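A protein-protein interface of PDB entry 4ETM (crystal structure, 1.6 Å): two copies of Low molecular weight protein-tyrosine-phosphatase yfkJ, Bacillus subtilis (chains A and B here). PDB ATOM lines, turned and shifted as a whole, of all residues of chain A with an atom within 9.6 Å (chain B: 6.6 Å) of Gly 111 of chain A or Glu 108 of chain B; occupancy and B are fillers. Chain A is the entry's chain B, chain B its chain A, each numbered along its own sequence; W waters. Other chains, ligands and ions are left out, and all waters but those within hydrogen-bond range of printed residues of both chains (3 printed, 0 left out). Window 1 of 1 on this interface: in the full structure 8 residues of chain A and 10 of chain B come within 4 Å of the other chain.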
ATOM      1  N   VAL A  24      -5.709 -32.399  25.494  1.00  0.00           N
ATOM      2  CA  VAL A  24      -5.177 -32.102  26.815  1.00  0.00           C
ATOM      3  C   VAL A  24      -6.042 -31.094  27.545  1.00  0.00           C
ATOM      4  O   VAL A  24      -6.353 -30.028  27.010  1.00  0.00           O
ATOM      5  CB  VAL A  24      -3.736 -31.557  26.749  1.00  0.00           C
ATOM      6  CG1 VAL A  24      -3.229 -31.259  28.143  1.00  0.00           C
ATOM      7  CG2 VAL A  24      -2.815 -32.555  26.042  1.00  0.00           C
ATOM      8  N   ILE A  59      -2.923 -32.106  32.478  1.00  0.00           N
ATOM      9  CA  ILE A  59      -1.805 -31.446  33.118  1.00  0.00           C
ATOM     10  C   ILE A  59      -1.634 -31.895  34.575  1.00  0.00           C
ATOM     11  O   ILE A  59      -0.507 -32.157  35.016  1.00  0.00           O
ATOM     12  CB  ILE A  59      -1.981 -29.914  33.067  1.00  0.00           C
ATOM     13  CG1 ILE A  59      -2.040 -29.428  31.609  1.00  0.00           C
ATOM     14  CG2 ILE A  59      -0.897 -29.236  33.883  1.00  0.00           C
ATOM     15  CD1 ILE A  59      -0.897 -29.955  30.749  1.00  0.00           C
ATOM     16  N   LEU A  96       4.805 -35.156  23.992  1.00  0.00           N
ATOM     17  CA  LEU A  96       5.089 -34.072  23.051  1.00  0.00           C
ATOM     18  C   LEU A  96       5.760 -34.581  21.788  1.00  0.00           C
ATOM     19  O   LEU A  96       5.529 -34.055  20.716  1.00  0.00           O
ATOM     20  CB  LEU A  96       5.971 -33.003  23.697  1.00  0.00           C
ATOM     21  CG  LEU A  96       5.439 -32.360  24.978  1.00  0.00           C
ATOM     22  CD1 LEU A  96       6.509 -31.523  25.626  1.00  0.00           C
ATOM     23  CD2 LEU A  96       4.224 -31.510  24.679  1.00  0.00           C
ATOM     24  N   ALA A 104      -4.951 -28.547  23.042  1.00  0.00           N
ATOM     25  CA  ALA A 104      -5.286 -28.055  24.376  1.00  0.00           C
ATOM     26  C   ALA A 104      -6.704 -27.534  24.410  1.00  0.00           C
ATOM     27  O   ALA A 104      -7.240 -27.091  23.391  1.00  0.00           O
ATOM     28  CB  ALA A 104      -4.354 -26.939  24.736  1.00  0.00           C
ATOM     29  N   MET A 105      -7.297 -27.542  25.596  1.00  0.00           N
ATOM     30  CA  MET A 105      -8.644 -27.014  25.742  1.00  0.00           C
ATOM     31  C   MET A 105      -8.663 -25.508  25.995  1.00  0.00           C
ATOM     32  O   MET A 105      -9.537 -24.804  25.501  1.00  0.00           O
ATOM     33  CB  MET A 105      -9.376 -27.730  26.865  1.00  0.00           C
ATOM     34  CG  MET A 105      -9.589 -29.186  26.590  1.00  0.00           C
ATOM     35  SD  MET A 105     -10.728 -29.484  25.214  1.00  0.00           S
ATOM     36  CE  MET A 105      -9.668 -30.364  24.074  1.00  0.00           C
ATOM     37  N   ASP A 106      -7.680 -25.016  26.750  1.00  0.00           N
ATOM     38  CA  ASP A 106      -7.646 -23.596  27.113  1.00  0.00           C
ATOM     39  C   ASP A 106      -6.231 -23.042  27.192  1.00  0.00           C
ATOM     40  O   ASP A 106      -5.259 -23.794  27.061  1.00  0.00           O
ATOM     41  CB  ASP A 106      -8.457 -23.308  28.393  1.00  0.00           C
ATOM     42  CG  ASP A 106      -7.878 -23.951  29.641  1.00  0.00           C
ATOM     43  OD1 ASP A 106      -6.646 -24.124  29.721  1.00  0.00           O
ATOM     44  OD2 ASP A 106      -8.670 -24.233  30.576  1.00  0.00           O
ATOM     45  N   ALA A 107      -6.124 -21.736  27.408  1.00  0.00           N
ATOM     46  CA  ALA A 107      -4.833 -21.052  27.412  1.00  0.00           C
ATOM     47  C   ALA A 107      -3.939 -21.512  28.569  1.00  0.00           C
ATOM     48  O   ALA A 107      -2.706 -21.534  28.431  1.00  0.00           O
ATOM     49  CB  ALA A 107      -5.038 -19.542  27.461  1.00  0.00           C
ATOM     50  N   GLU A 108      -4.549 -21.861  29.701  1.00  0.00           N
ATOM     51  CA  GLU A 108      -3.770 -22.381  30.823  1.00  0.00           C
ATOM     52  C   GLU A 108      -3.079 -23.663  30.373  1.00  0.00           C
ATOM     53  O   GLU A 108      -1.885 -23.844  30.612  1.00  0.00           O
ATOM     54  CB  GLU A 108      -4.629 -22.637  32.055  1.00  0.00           C
ATOM     55  CG  GLU A 108      -5.088 -21.343  32.715  1.00  0.00           C
ATOM     56  CD  GLU A 108      -5.775 -21.562  34.056  1.00  0.00           C
ATOM     57  OE1 GLU A 108      -5.676 -22.671  34.623  1.00  0.00           O
ATOM     58  OE2 GLU A 108      -6.422 -20.617  34.549  1.00  0.00           O
ATOM     59  N   ASN A 109      -3.826 -24.547  29.705  1.00  0.00           N
ATOM     60  CA  ASN A 109      -3.249 -25.799  29.208  1.00  0.00           C
ATOM     61  C   ASN A 109      -2.086 -25.536  28.239  1.00  0.00           C
ATOM     62  O   ASN A 109      -1.064 -26.211  28.283  1.00  0.00           O
ATOM     63  CB  ASN A 109      -4.272 -26.665  28.461  1.00  0.00           C
ATOM     64  CG  ASN A 109      -5.526 -26.998  29.262  1.00  0.00           C
ATOM     65  OD1 ASN A 109      -6.587 -27.170  28.661  1.00  0.00           O
ATOM     66  ND2 ASN A 109      -5.424 -27.102  30.588  1.00  0.00           N
ATOM     67  N   ILE A 110      -2.249 -24.541  27.365  1.00  0.00           N
ATOM     68  CA  ILE A 110      -1.184 -24.146  26.456  1.00  0.00           C
ATOM     69  C   ILE A 110       0.082 -23.727  27.203  1.00  0.00           C
ATOM     70  O   ILE A 110       1.198 -24.143  26.861  1.00  0.00           O
ATOM     71  CB  ILE A 110      -1.606 -22.990  25.554  1.00  0.00           C
ATOM     72  CG1 ILE A 110      -2.710 -23.431  24.581  1.00  0.00           C
ATOM     73  CG2 ILE A 110      -0.379 -22.450  24.833  1.00  0.00           C
ATOM     74  CD1 ILE A 110      -2.258 -24.356  23.444  1.00  0.00           C
ATOM     75  N   GLY A 111      -0.105 -22.904  28.230  1.00  0.00           N
ATOM     76  CA  GLY A 111       1.003 -22.485  29.074  1.00  0.00           C
ATOM     77  C   GLY A 111       1.706 -23.666  29.726  1.00  0.00           C
ATOM     78  O   GLY A 111       2.940 -23.705  29.793  1.00  0.00           O
ATOM     79  N   SER A 112       0.921 -24.627  30.201  1.00  0.00           N
ATOM     80  CA  SER A 112       1.505 -25.816  30.812  1.00  0.00           C
ATOM     81  C   SER A 112       2.350 -26.590  29.824  1.00  0.00           C
ATOM     82  O   SER A 112       3.451 -27.023  30.141  1.00  0.00           O
ATOM     83  CB  SER A 112       0.422 -26.741  31.347  1.00  0.00           C
ATOM     84  OG  SER A 112      -0.383 -26.093  32.310  1.00  0.00           O
ATOM     85  N   LEU A 113       1.809 -26.757  28.625  1.00  0.00           N
ATOM     86  CA  LEU A 113       2.435 -27.602  27.609  1.00  0.00           C
ATOM     87  C   LEU A 113       3.709 -26.962  27.063  1.00  0.00           C
ATOM     88  O   LEU A 113       4.728 -27.632  26.901  1.00  0.00           O
ATOM     89  CB  LEU A 113       1.433 -27.906  26.500  1.00  0.00           C
ATOM     90  CG  LEU A 113       0.295 -28.849  26.926  1.00  0.00           C
ATOM     91  CD1 LEU A 113      -0.834 -28.772  25.924  1.00  0.00           C
ATOM     92  CD2 LEU A 113       0.782 -30.303  27.076  1.00  0.00           C
ATOM     93  N   ARG A 114       3.666 -25.654  26.834  1.00  0.00           N
ATOM     94  CA  ARG A 114       4.858 -24.955  26.348  1.00  0.00           C
ATOM     95  C   ARG A 114       5.980 -24.968  27.373  1.00  0.00           C
ATOM     96  O   ARG A 114       7.146 -25.146  27.012  1.00  0.00           O
ATOM     97  CB  ARG A 114       4.535 -23.513  25.947  1.00  0.00           C
ATOM     98  CG  ARG A 114       3.661 -23.401  24.699  1.00  0.00           C
ATOM     99  CD  ARG A 114       3.346 -21.922  24.381  1.00  0.00           C
ATOM    100  NE  ARG A 114       2.506 -21.828  23.187  1.00  0.00           N
ATOM    101  CZ  ARG A 114       1.905 -20.715  22.778  1.00  0.00           C
ATOM    102  NH1 ARG A 114       2.044 -19.585  23.465  1.00  0.00           N
ATOM    103  NH2 ARG A 114       1.160 -20.736  21.680  1.00  0.00           N
ATOM    104  N   SER A 115       5.637 -24.765  28.644  1.00  0.00           N
ATOM    105  CA  SER A 115       6.639 -24.814  29.712  1.00  0.00           C
ATOM    106  C   SER A 115       7.250 -26.219  29.832  1.00  0.00           C
ATOM    107  O   SER A 115       8.474 -26.360  29.996  1.00  0.00           O
ATOM    108  CB  SER A 115       6.035 -24.340  31.050  1.00  0.00           C
ATOM    109  OG  SER A 115       6.956 -24.531  32.110  1.00  0.00           O
ATOM    110  N   MET A 116       6.410 -27.248  29.740  1.00  0.00           N
ATOM    111  CA  MET A 116       6.885 -28.635  29.764  1.00  0.00           C
ATOM    112  C   MET A 116       7.841 -28.890  28.607  1.00  0.00           C
ATOM    113  O   MET A 116       8.835 -29.610  28.745  1.00  0.00           O
ATOM    114  CB  MET A 116       5.709 -29.611  29.680  1.00  0.00           C
ATOM    115  CG  MET A 116       6.069 -31.015  30.088  1.00  0.00           C
ATOM    116  SD  MET A 116       4.662 -32.105  29.875  1.00  0.00           S
ATOM    117  CE  MET A 116       3.415 -31.059  30.589  1.00  0.00           C
ATOM    118  N   ALA A 117       7.542 -28.283  27.468  1.00  0.00           N
ATOM    119  CA  ALA A 117       8.355 -28.456  26.262  1.00  0.00           C
ATOM    120  C   ALA A 117       9.605 -27.580  26.252  1.00  0.00           C
ATOM    121  O   ALA A 117      10.388 -27.604  25.290  1.00  0.00           O
ATOM    122  CB  ALA A 117       7.522 -28.172  25.036  1.00  0.00           C
ATOM    123  N   GLY A 118       9.791 -26.801  27.314  1.00  0.00           N
ATOM    124  CA  GLY A 118      10.886 -25.855  27.388  1.00  0.00           C
ATOM    125  C   GLY A 118      10.824 -24.821  26.286  1.00  0.00           C
ATOM    126  O   GLY A 118      11.855 -24.332  25.847  1.00  0.00           O
ATOM    127  N   PHE A 119       9.613 -24.487  25.843  1.00  0.00           N
ATOM    128  CA  PHE A 119       9.400 -23.501  24.767  1.00  0.00           C
ATOM    129  C   PHE A 119      10.140 -23.829  23.471  1.00  0.00           C
ATOM    130  O   PHE A 119      10.487 -22.940  22.690  1.00  0.00           O
ATOM    131  CB  PHE A 119       9.686 -22.079  25.256  1.00  0.00           C
ATOM    132  CG  PHE A 119       8.782 -21.663  26.360  1.00  0.00           C
ATOM    133  CD1 PHE A 119       7.515 -21.183  26.086  1.00  0.00           C
ATOM    134  CD2 PHE A 119       9.166 -21.821  27.675  1.00  0.00           C
ATOM    135  CE1 PHE A 119       6.655 -20.842  27.103  1.00  0.00           C
ATOM    136  CE2 PHE A 119       8.315 -21.471  28.700  1.00  0.00           C
ATOM    137  CZ  PHE A 119       7.049 -20.984  28.412  1.00  0.00           C
ATOM    138  N   THR A 122       7.109 -26.435  19.643  1.00  0.00           N
ATOM    139  CA  THR A 122       5.727 -26.397  20.106  1.00  0.00           C
ATOM    140  C   THR A 122       4.710 -26.030  19.024  1.00  0.00           C
ATOM    141  O   THR A 122       3.537 -25.790  19.331  1.00  0.00           O
ATOM    142  CB  THR A 122       5.563 -25.404  21.275  1.00  0.00           C
ATOM    143  OG1 THR A 122       5.921 -24.094  20.830  1.00  0.00           O
ATOM    144  CG2 THR A 122       6.461 -25.788  22.442  1.00  0.00           C
ATOM    145  N   ILE A 125       1.305 -27.666  19.044  1.00  0.00           N
ATOM    146  CA  ILE A 125       0.462 -27.509  20.219  1.00  0.00           C
ATOM    147  C   ILE A 125      -0.455 -26.308  20.009  1.00  0.00           C
ATOM    148  O   ILE A 125       0.013 -25.168  19.984  1.00  0.00           O
ATOM    149  CB  ILE A 125       1.320 -27.274  21.474  1.00  0.00           C
ATOM    150  CG1 ILE A 125       2.378 -28.370  21.608  1.00  0.00           C
ATOM    151  CG2 ILE A 125       0.443 -27.189  22.729  1.00  0.00           C
ATOM    152  CD1 ILE A 125       3.355 -28.115  22.725  1.00  0.00           C
ATOM    153  N   LYS A 126      -1.754 -26.569  19.863  1.00  0.00           N
ATOM    154  CA  LYS A 126      -2.745 -25.526  19.570  1.00  0.00           C
ATOM    155  C   LYS A 126      -4.007 -25.762  20.376  1.00  0.00           C
ATOM    156  O   LYS A 126      -4.243 -26.889  20.827  1.00  0.00           O
ATOM    157  CB  LYS A 126      -3.106 -25.546  18.081  1.00  0.00           C
ATOM    158  CG  LYS A 126      -2.009 -25.040  17.184  1.00  0.00           C
ATOM    159  CD  LYS A 126      -2.442 -25.018  15.726  1.00  0.00           C
ATOM    160  CE  LYS A 126      -1.460 -24.217  14.879  1.00  0.00           C
ATOM    161  NZ  LYS A 126      -0.127 -24.884  14.787  1.00  0.00           N
ATOM    162  N   ARG A 127      -4.814 -24.719  20.573  1.00  0.00           N
ATOM    163  CA  ARG A 127      -6.109 -24.878  21.238  1.00  0.00           C
ATOM    164  C   ARG A 127      -7.145 -25.467  20.284  1.00  0.00           C
ATOM    165  O   ARG A 127      -7.113 -25.187  19.079  1.00  0.00           O
ATOM    166  CB  ARG A 127      -6.614 -23.555  21.825  1.00  0.00           C
ATOM    167  CG  ARG A 127      -5.861 -23.140  23.081  1.00  0.00           C
ATOM    168  CD  ARG A 127      -6.381 -21.853  23.659  1.00  0.00           C
ATOM    169  NE  ARG A 127      -6.184 -20.744  22.739  1.00  0.00           N
ATOM    170  CZ  ARG A 127      -6.536 -19.489  23.003  1.00  0.00           C
ATOM    171  NH1 ARG A 127      -7.111 -19.173  24.163  1.00  0.00           N
ATOM    172  NH2 ARG A 127      -6.313 -18.545  22.100  1.00  0.00           N
ATOM    173  N   ASP A 130      -8.907 -23.009  18.145  1.00  0.00           N
ATOM    174  CA  ASP A 130      -8.095 -22.447  17.047  1.00  0.00           C
ATOM    175  C   ASP A 130      -8.597 -22.940  15.691  1.00  0.00           C
ATOM    176  O   ASP A 130      -8.413 -22.272  14.673  1.00  0.00           O
ATOM    177  CB  ASP A 130      -6.621 -22.846  17.168  1.00  0.00           C
ATOM    178  CG  ASP A 130      -5.892 -22.113  18.278  1.00  0.00           C
ATOM    179  OD1 ASP A 130      -6.518 -21.339  19.034  1.00  0.00           O
ATOM    180  OD2 ASP A 130      -4.667 -22.328  18.397  1.00  0.00           O
ATOM    181  N   ALA A 138     -12.204 -18.591  22.619  1.00  0.00           N
ATOM    182  CA  ALA A 138     -10.907 -19.202  22.368  1.00  0.00           C
ATOM    183  C   ALA A 138     -10.676 -20.420  23.263  1.00  0.00           C
ATOM    184  O   ALA A 138      -9.880 -21.300  22.914  1.00  0.00           O
ATOM    185  CB  ALA A 138      -9.814 -18.191  22.583  1.00  0.00           C
ATOM    186  N   ASP A 139     -11.355 -20.448  24.413  1.00  0.00           N
ATOM    187  CA  ASP A 139     -11.170 -21.479  25.435  1.00  0.00           C
ATOM    188  C   ASP A 139     -12.430 -22.312  25.653  1.00  0.00           C
ATOM    189  O   ASP A 139     -13.531 -21.776  25.712  1.00  0.00           O
ATOM    190  CB  ASP A 139     -10.819 -20.830  26.778  1.00  0.00           C
ATOM    191  CG  ASP A 139      -9.493 -20.102  26.750  1.00  0.00           C
ATOM    192  OD1 ASP A 139      -8.520 -20.652  26.213  1.00  0.00           O
ATOM    193  OD2 ASP A 139      -9.426 -18.967  27.265  1.00  0.00           O
ATOM    194  N   LEU B  26       6.035 -14.020  31.313  1.00  0.00           N
ATOM    195  CA  LEU B  26       6.774 -14.990  30.513  1.00  0.00           C
ATOM    196  C   LEU B  26       8.277 -14.734  30.536  1.00  0.00           C
ATOM    197  O   LEU B  26       9.062 -15.621  30.903  1.00  0.00           O
ATOM    198  CB  LEU B  26       6.239 -14.973  29.075  1.00  0.00           C
ATOM    199  CG  LEU B  26       6.946 -15.913  28.099  1.00  0.00           C
ATOM    200  CD1 LEU B  26       6.769 -17.336  28.552  1.00  0.00           C
ATOM    201  CD2 LEU B  26       6.395 -15.711  26.681  1.00  0.00           C
ATOM    202  N   ILE B  59       8.390 -17.153  33.634  1.00  0.00           N
ATOM    203  CA  ILE B  59       8.256 -18.553  33.294  1.00  0.00           C
ATOM    204  C   ILE B  59       9.471 -19.072  32.520  1.00  0.00           C
ATOM    205  O   ILE B  59       9.983 -20.163  32.820  1.00  0.00           O
ATOM    206  CB  ILE B  59       6.982 -18.820  32.475  1.00  0.00           C
ATOM    207  CG1 ILE B  59       5.735 -18.441  33.282  1.00  0.00           C
ATOM    208  CG2 ILE B  59       6.932 -20.301  32.117  1.00  0.00           C
ATOM    209  CD1 ILE B  59       5.652 -19.138  34.632  1.00  0.00           C
ATOM    210  N   ASP B 106      -1.061 -13.428  32.691  1.00  0.00           N
ATOM    211  CA  ASP B 106      -2.063 -14.052  31.829  1.00  0.00           C
ATOM    212  C   ASP B 106      -2.305 -15.534  32.116  1.00  0.00           C
ATOM    213  O   ASP B 106      -1.659 -16.140  32.996  1.00  0.00           O
ATOM    214  CB  ASP B 106      -1.739 -13.821  30.345  1.00  0.00           C
ATOM    215  CG  ASP B 106      -0.460 -14.504  29.897  1.00  0.00           C
ATOM    216  OD1 ASP B 106      -0.153 -15.615  30.357  1.00  0.00           O
ATOM    217  OD2 ASP B 106       0.243 -13.941  29.041  1.00  0.00           O
ATOM    218  N   ALA B 107      -3.256 -16.106  31.384  1.00  0.00           N
ATOM    219  CA  ALA B 107      -3.716 -17.457  31.654  1.00  0.00           C
ATOM    220  C   ALA B 107      -2.611 -18.453  31.334  1.00  0.00           C
ATOM    221  O   ALA B 107      -2.421 -19.432  32.060  1.00  0.00           O
ATOM    222  CB  ALA B 107      -4.984 -17.770  30.862  1.00  0.00           C
ATOM    223  N   GLU B 108      -1.865 -18.206  30.264  1.00  0.00           N
ATOM    224  CA  GLU B 108      -0.723 -19.079  29.982  1.00  0.00           C
ATOM    225  C   GLU B 108       0.255 -19.154  31.149  1.00  0.00           C
ATOM    226  O   GLU B 108       0.764 -20.234  31.473  1.00  0.00           O
ATOM    227  CB  GLU B 108      -0.014 -18.697  28.673  1.00  0.00           C
ATOM    228  CG  GLU B 108      -0.883 -18.932  27.444  1.00  0.00           C
ATOM    229  CD  GLU B 108      -0.206 -18.495  26.149  1.00  0.00           C
ATOM    230  OE1 GLU B 108       0.816 -17.785  26.219  1.00  0.00           O
ATOM    231  OE2 GLU B 108      -0.696 -18.851  25.059  1.00  0.00           O
ATOM    232  N   ASN B 109       0.531 -18.010  31.762  1.00  0.00           N
ATOM    233  CA  ASN B 109       1.443 -17.963  32.905  1.00  0.00           C
ATOM    234  C   ASN B 109       0.921 -18.840  34.044  1.00  0.00           C
ATOM    235  O   ASN B 109       1.686 -19.572  34.693  1.00  0.00           O
ATOM    236  CB  ASN B 109       1.580 -16.539  33.445  1.00  0.00           C
ATOM    237  CG  ASN B 109       2.185 -15.567  32.456  1.00  0.00           C
ATOM    238  OD1 ASN B 109       1.940 -14.368  32.556  1.00  0.00           O
ATOM    239  ND2 ASN B 109       2.989 -16.052  31.532  1.00  0.00           N
ATOM    240  N   ILE B 110      -0.384 -18.753  34.294  1.00  0.00           N
ATOM    241  CA  ILE B 110      -1.020 -19.553  35.338  1.00  0.00           C
ATOM    242  C   ILE B 110      -0.814 -21.033  35.037  1.00  0.00           C
ATOM    243  O   ILE B 110      -0.420 -21.808  35.909  1.00  0.00           O
ATOM    244  CB  ILE B 110      -2.528 -19.276  35.428  1.00  0.00           C
ATOM    245  CG1 ILE B 110      -2.797 -17.813  35.803  1.00  0.00           C
ATOM    246  CG2 ILE B 110      -3.209 -20.277  36.355  1.00  0.00           C
ATOM    247  CD1 ILE B 110      -2.832 -17.542  37.278  1.00  0.00           C
ATOM    248  N   GLY B 111      -1.060 -21.414  33.788  1.00  0.00           N
ATOM    249  CA  GLY B 111      -0.893 -22.791  33.373  1.00  0.00           C
ATOM    250  C   GLY B 111       0.536 -23.276  33.536  1.00  0.00           C
ATOM    251  O   GLY B 111       0.762 -24.413  33.946  1.00  0.00           O
ATOM    252  N   SER B 112       1.502 -22.415  33.216  1.00  0.00           N
ATOM    253  CA  SER B 112       2.902 -22.778  33.388  1.00  0.00           C
ATOM    254  C   SER B 112       3.242 -23.016  34.845  1.00  0.00           C
ATOM    255  O   SER B 112       3.967 -23.957  35.154  1.00  0.00           O
ATOM    256  CB  SER B 112       3.825 -21.713  32.804  1.00  0.00           C
ATOM    257  OG  SER B 112       3.631 -21.607  31.403  1.00  0.00           O
ATOM    258  N   LEU B 113       2.717 -22.168  35.734  1.00  0.00           N
ATOM    259  CA  LEU B 113       2.972 -22.321  37.161  1.00  0.00           C
ATOM    260  C   LEU B 113       2.326 -23.625  37.645  1.00  0.00           C
ATOM    261  O   LEU B 113       2.850 -24.295  38.528  1.00  0.00           O
ATOM    262  CB  LEU B 113       2.475 -21.099  37.952  1.00  0.00           C
ATOM    263  CG  LEU B 113       3.237 -19.787  37.710  1.00  0.00           C
ATOM    264  CD1 LEU B 113       2.453 -18.572  38.188  1.00  0.00           C
ATOM    265  CD2 LEU B 113       4.607 -19.803  38.371  1.00  0.00           C
ATOM    266  N   SER B 115       1.944 -26.455  35.898  1.00  0.00           N
ATOM    267  CA  SER B 115       2.834 -27.515  35.450  1.00  0.00           C
ATOM    268  C   SER B 115       4.059 -27.641  36.369  1.00  0.00           C
ATOM    269  O   SER B 115       4.663 -28.709  36.480  1.00  0.00           O
ATOM    270  CB  SER B 115       3.285 -27.221  34.008  1.00  0.00           C
ATOM    271  OG  SER B 115       4.079 -28.267  33.462  1.00  0.00           O
ATOM    272  N   ARG B 127      -4.481 -14.310  38.361  1.00  0.00           N
ATOM    273  CA  ARG B 127      -4.096 -13.281  37.391  1.00  0.00           C
ATOM    274  C   ARG B 127      -4.268 -11.881  37.987  1.00  0.00           C
ATOM    275  O   ARG B 127      -5.176 -11.651  38.793  1.00  0.00           O
ATOM    276  CB  ARG B 127      -4.917 -13.383  36.097  1.00  0.00           C
ATOM    277  CG  ARG B 127      -4.551 -14.565  35.221  1.00  0.00           C
ATOM    278  CD  ARG B 127      -5.392 -14.583  33.948  1.00  0.00           C
ATOM    279  NE  ARG B 127      -6.821 -14.678  34.234  1.00  0.00           N
ATOM    280  CZ  ARG B 127      -7.739 -14.908  33.303  1.00  0.00           C
ATOM    281  NH1 ARG B 127      -7.368 -15.055  32.036  1.00  0.00           N
ATOM    282  NH2 ARG B 127      -9.026 -14.995  33.633  1.00  0.00           N
ATOM    283  N   ASP B 139      -6.458 -10.888  30.551  1.00  0.00           N
ATOM    284  CA  ASP B 139      -5.029 -11.108  30.373  1.00  0.00           C
ATOM    285  C   ASP B 139      -4.301  -9.809  30.075  1.00  0.00           C
ATOM    286  O   ASP B 139      -4.780  -8.994  29.291  1.00  0.00           O
ATOM    287  CB  ASP B 139      -4.791 -12.098  29.233  1.00  0.00           C
ATOM    288  CG  ASP B 139      -5.397 -13.455  29.509  1.00  0.00           C
ATOM    289  OD1 ASP B 139      -5.153 -14.000  30.602  1.00  0.00           O
ATOM    290  OD2 ASP B 139      -6.141 -13.966  28.642  1.00  0.00           O
HETATM  291  O   HOH W   1      -6.423 -18.080  34.116  1.00  0.00           O
HETATM  292  O   HOH W   2       9.190 -22.741  32.034  1.00  0.00           O
HETATM  293  O   HOH W   3       6.604 -27.069  33.125  1.00  0.00           O
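O of Gly 111 of chain B lies within hydrogen-bond range of OG of Ser 112 of chain A (2.6 Å).
OE2 of Glu 108 of chain B is in salt-bridge range of NH1 of Arg 114 of chain A, at 3.3 Å.
The backbone carbonyl oxygen (O) of Gly 111 of chain A is in hydrogen-bond range of the side-chain hydroxyl (OG) of Ser 112 of chain B (2.7 Å).
O of Leu 26 of chain B is in hydrogen-bond range of N of Ile 59 of chain B (3.2 Å).
The side-chain carboxylate (OD1) of Asp 106 of chain A is in hydrogen-bond range of the backbone NH (N) of Glu 108 of chain A (3.1 Å).
The side-chain carboxylate of Asp 139 of chain A sits at hydrogen-bond distance from the backbone NH of Ala 107 of chain A, at 2.9 Å.
O of Glu 108 of chain B is in hydrogen-bond range of OG of Ser 112 of chain B.
The backbone carbonyl oxygen of Glu 108 of chain A sits at hydrogen-bond distance from the side-chain hydroxyl of Ser 112 of chain A (3.2 Å).
The backbone NH of Ala 107 of chain B is in hydrogen-bond range of the side-chain carboxylate of Asp 139 of chain B.
Ala 107 of chain A touches Ala 107 of chain B (CB to CB, 3.8 Å).
CD of Glu 108 of chain A touches CG2 of Ile 110 of chain B, 3.7 Å away.
CA of Gly 111 of chain B touches O of Glu 108 of chain A (3.1 Å).
Ile 110 of chain A touches Glu 108 of chain B.
Gly 111 of chain A touches Glu 108 of chain B.
Ser 112 of chain B touches Ser 112 of chain A (N to N, 3.8 Å).
Ser 115 of chain B touches Ser 112 of chain A (OG to O, 3.6 Å).
Ser 115 of chain A touches Ser 112 of chain B (CB to OG, 3.7 Å).
Leu 26 of chain B touches Phe 119 of chain A.
Phe 119 of chain A touches Ile 59 of chain B.
Of the printed residues of chain B, Glu 108 of chain A touches Ala 107 (3.3 Å), Ile 110 (3.7 Å) and Gly 111 (3.1 Å).
Of the printed residues of chain B, Gly 111 of chain A touches Glu 108 (3.3 Å) and Ser 112 (2.7 Å).
Of the printed residues of chain B, Ser 112 of chain A touches Gly 111, Ser 112 and Ser 115.
Leu 113 of chain A touches none of the printed residues of chain B.
Of the printed residues of chain B, Arg 114 of chain A touches Glu 108 (3.3 Å).
Printed residues of chain A within 4 Å of Ile 59 of chain B: Phe 119 (3.8 Å).
Of the printed residues of chain A, Ala 107 of chain B touches Ala 107 and Glu 108.
No residue of chain A comes within 4 Å of Asn 109 of chain B.
Ser 112 of chain B touches just these residues of chain A: Gly 111, Ser 112 and Ser 115.
The nearest printed residue of chain B that does not touch Phe 119 of chain A is Ser 112 of chain B (4.6 Å).
Of the 13 printed residues of chain B, 8 touch a printed residue of chain A.
Hydrophobic or aromatic side chains of chain B within 4 Å of the printed part of chain A: Leu 26, Ile 59, Ala 107 and Ile 110.
Among the printed residues, 15 pairs touch across the chains.
Ala 107 of chain A touches its own counterpart, Ala 107 of chain B.
Ala 107 of chain A touches Glu 108 of chain B, and with the chains exchanged Glu 108 of chain A touches Ala 107 of chain B.
Glu 108 of chain A touches Ile 110 of chain B, and with the chains exchanged Ile 110 of chain A touches Glu 108 of chain B.
Glu 108 of chain A touches Gly 111 of chain B, and with the chains exchanged Gly 111 of chain A touches Glu 108 of chain B.
Water W1 bridges OE2 of Glu 108 of chain A (2.6 Å) and NE of Arg 127 of chain B (3.4 Å).
Water W3 lies within hydrogen-bond range of the side-chain hydroxyl (OG) of Ser 115 of chain A (2.8 Å), the side-chain hydroxyl (OG) of Ser 115 of chain B (2.8 Å) and the backbone NH (N) of Met 116 of chain A (3.4 Å).
Water W2 lies within hydrogen-bond range of the backbone carbonyl oxygen (O) of Ile 59 of chain B and the side-chain hydroxyl (OG) of Ser 115 of chain A.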
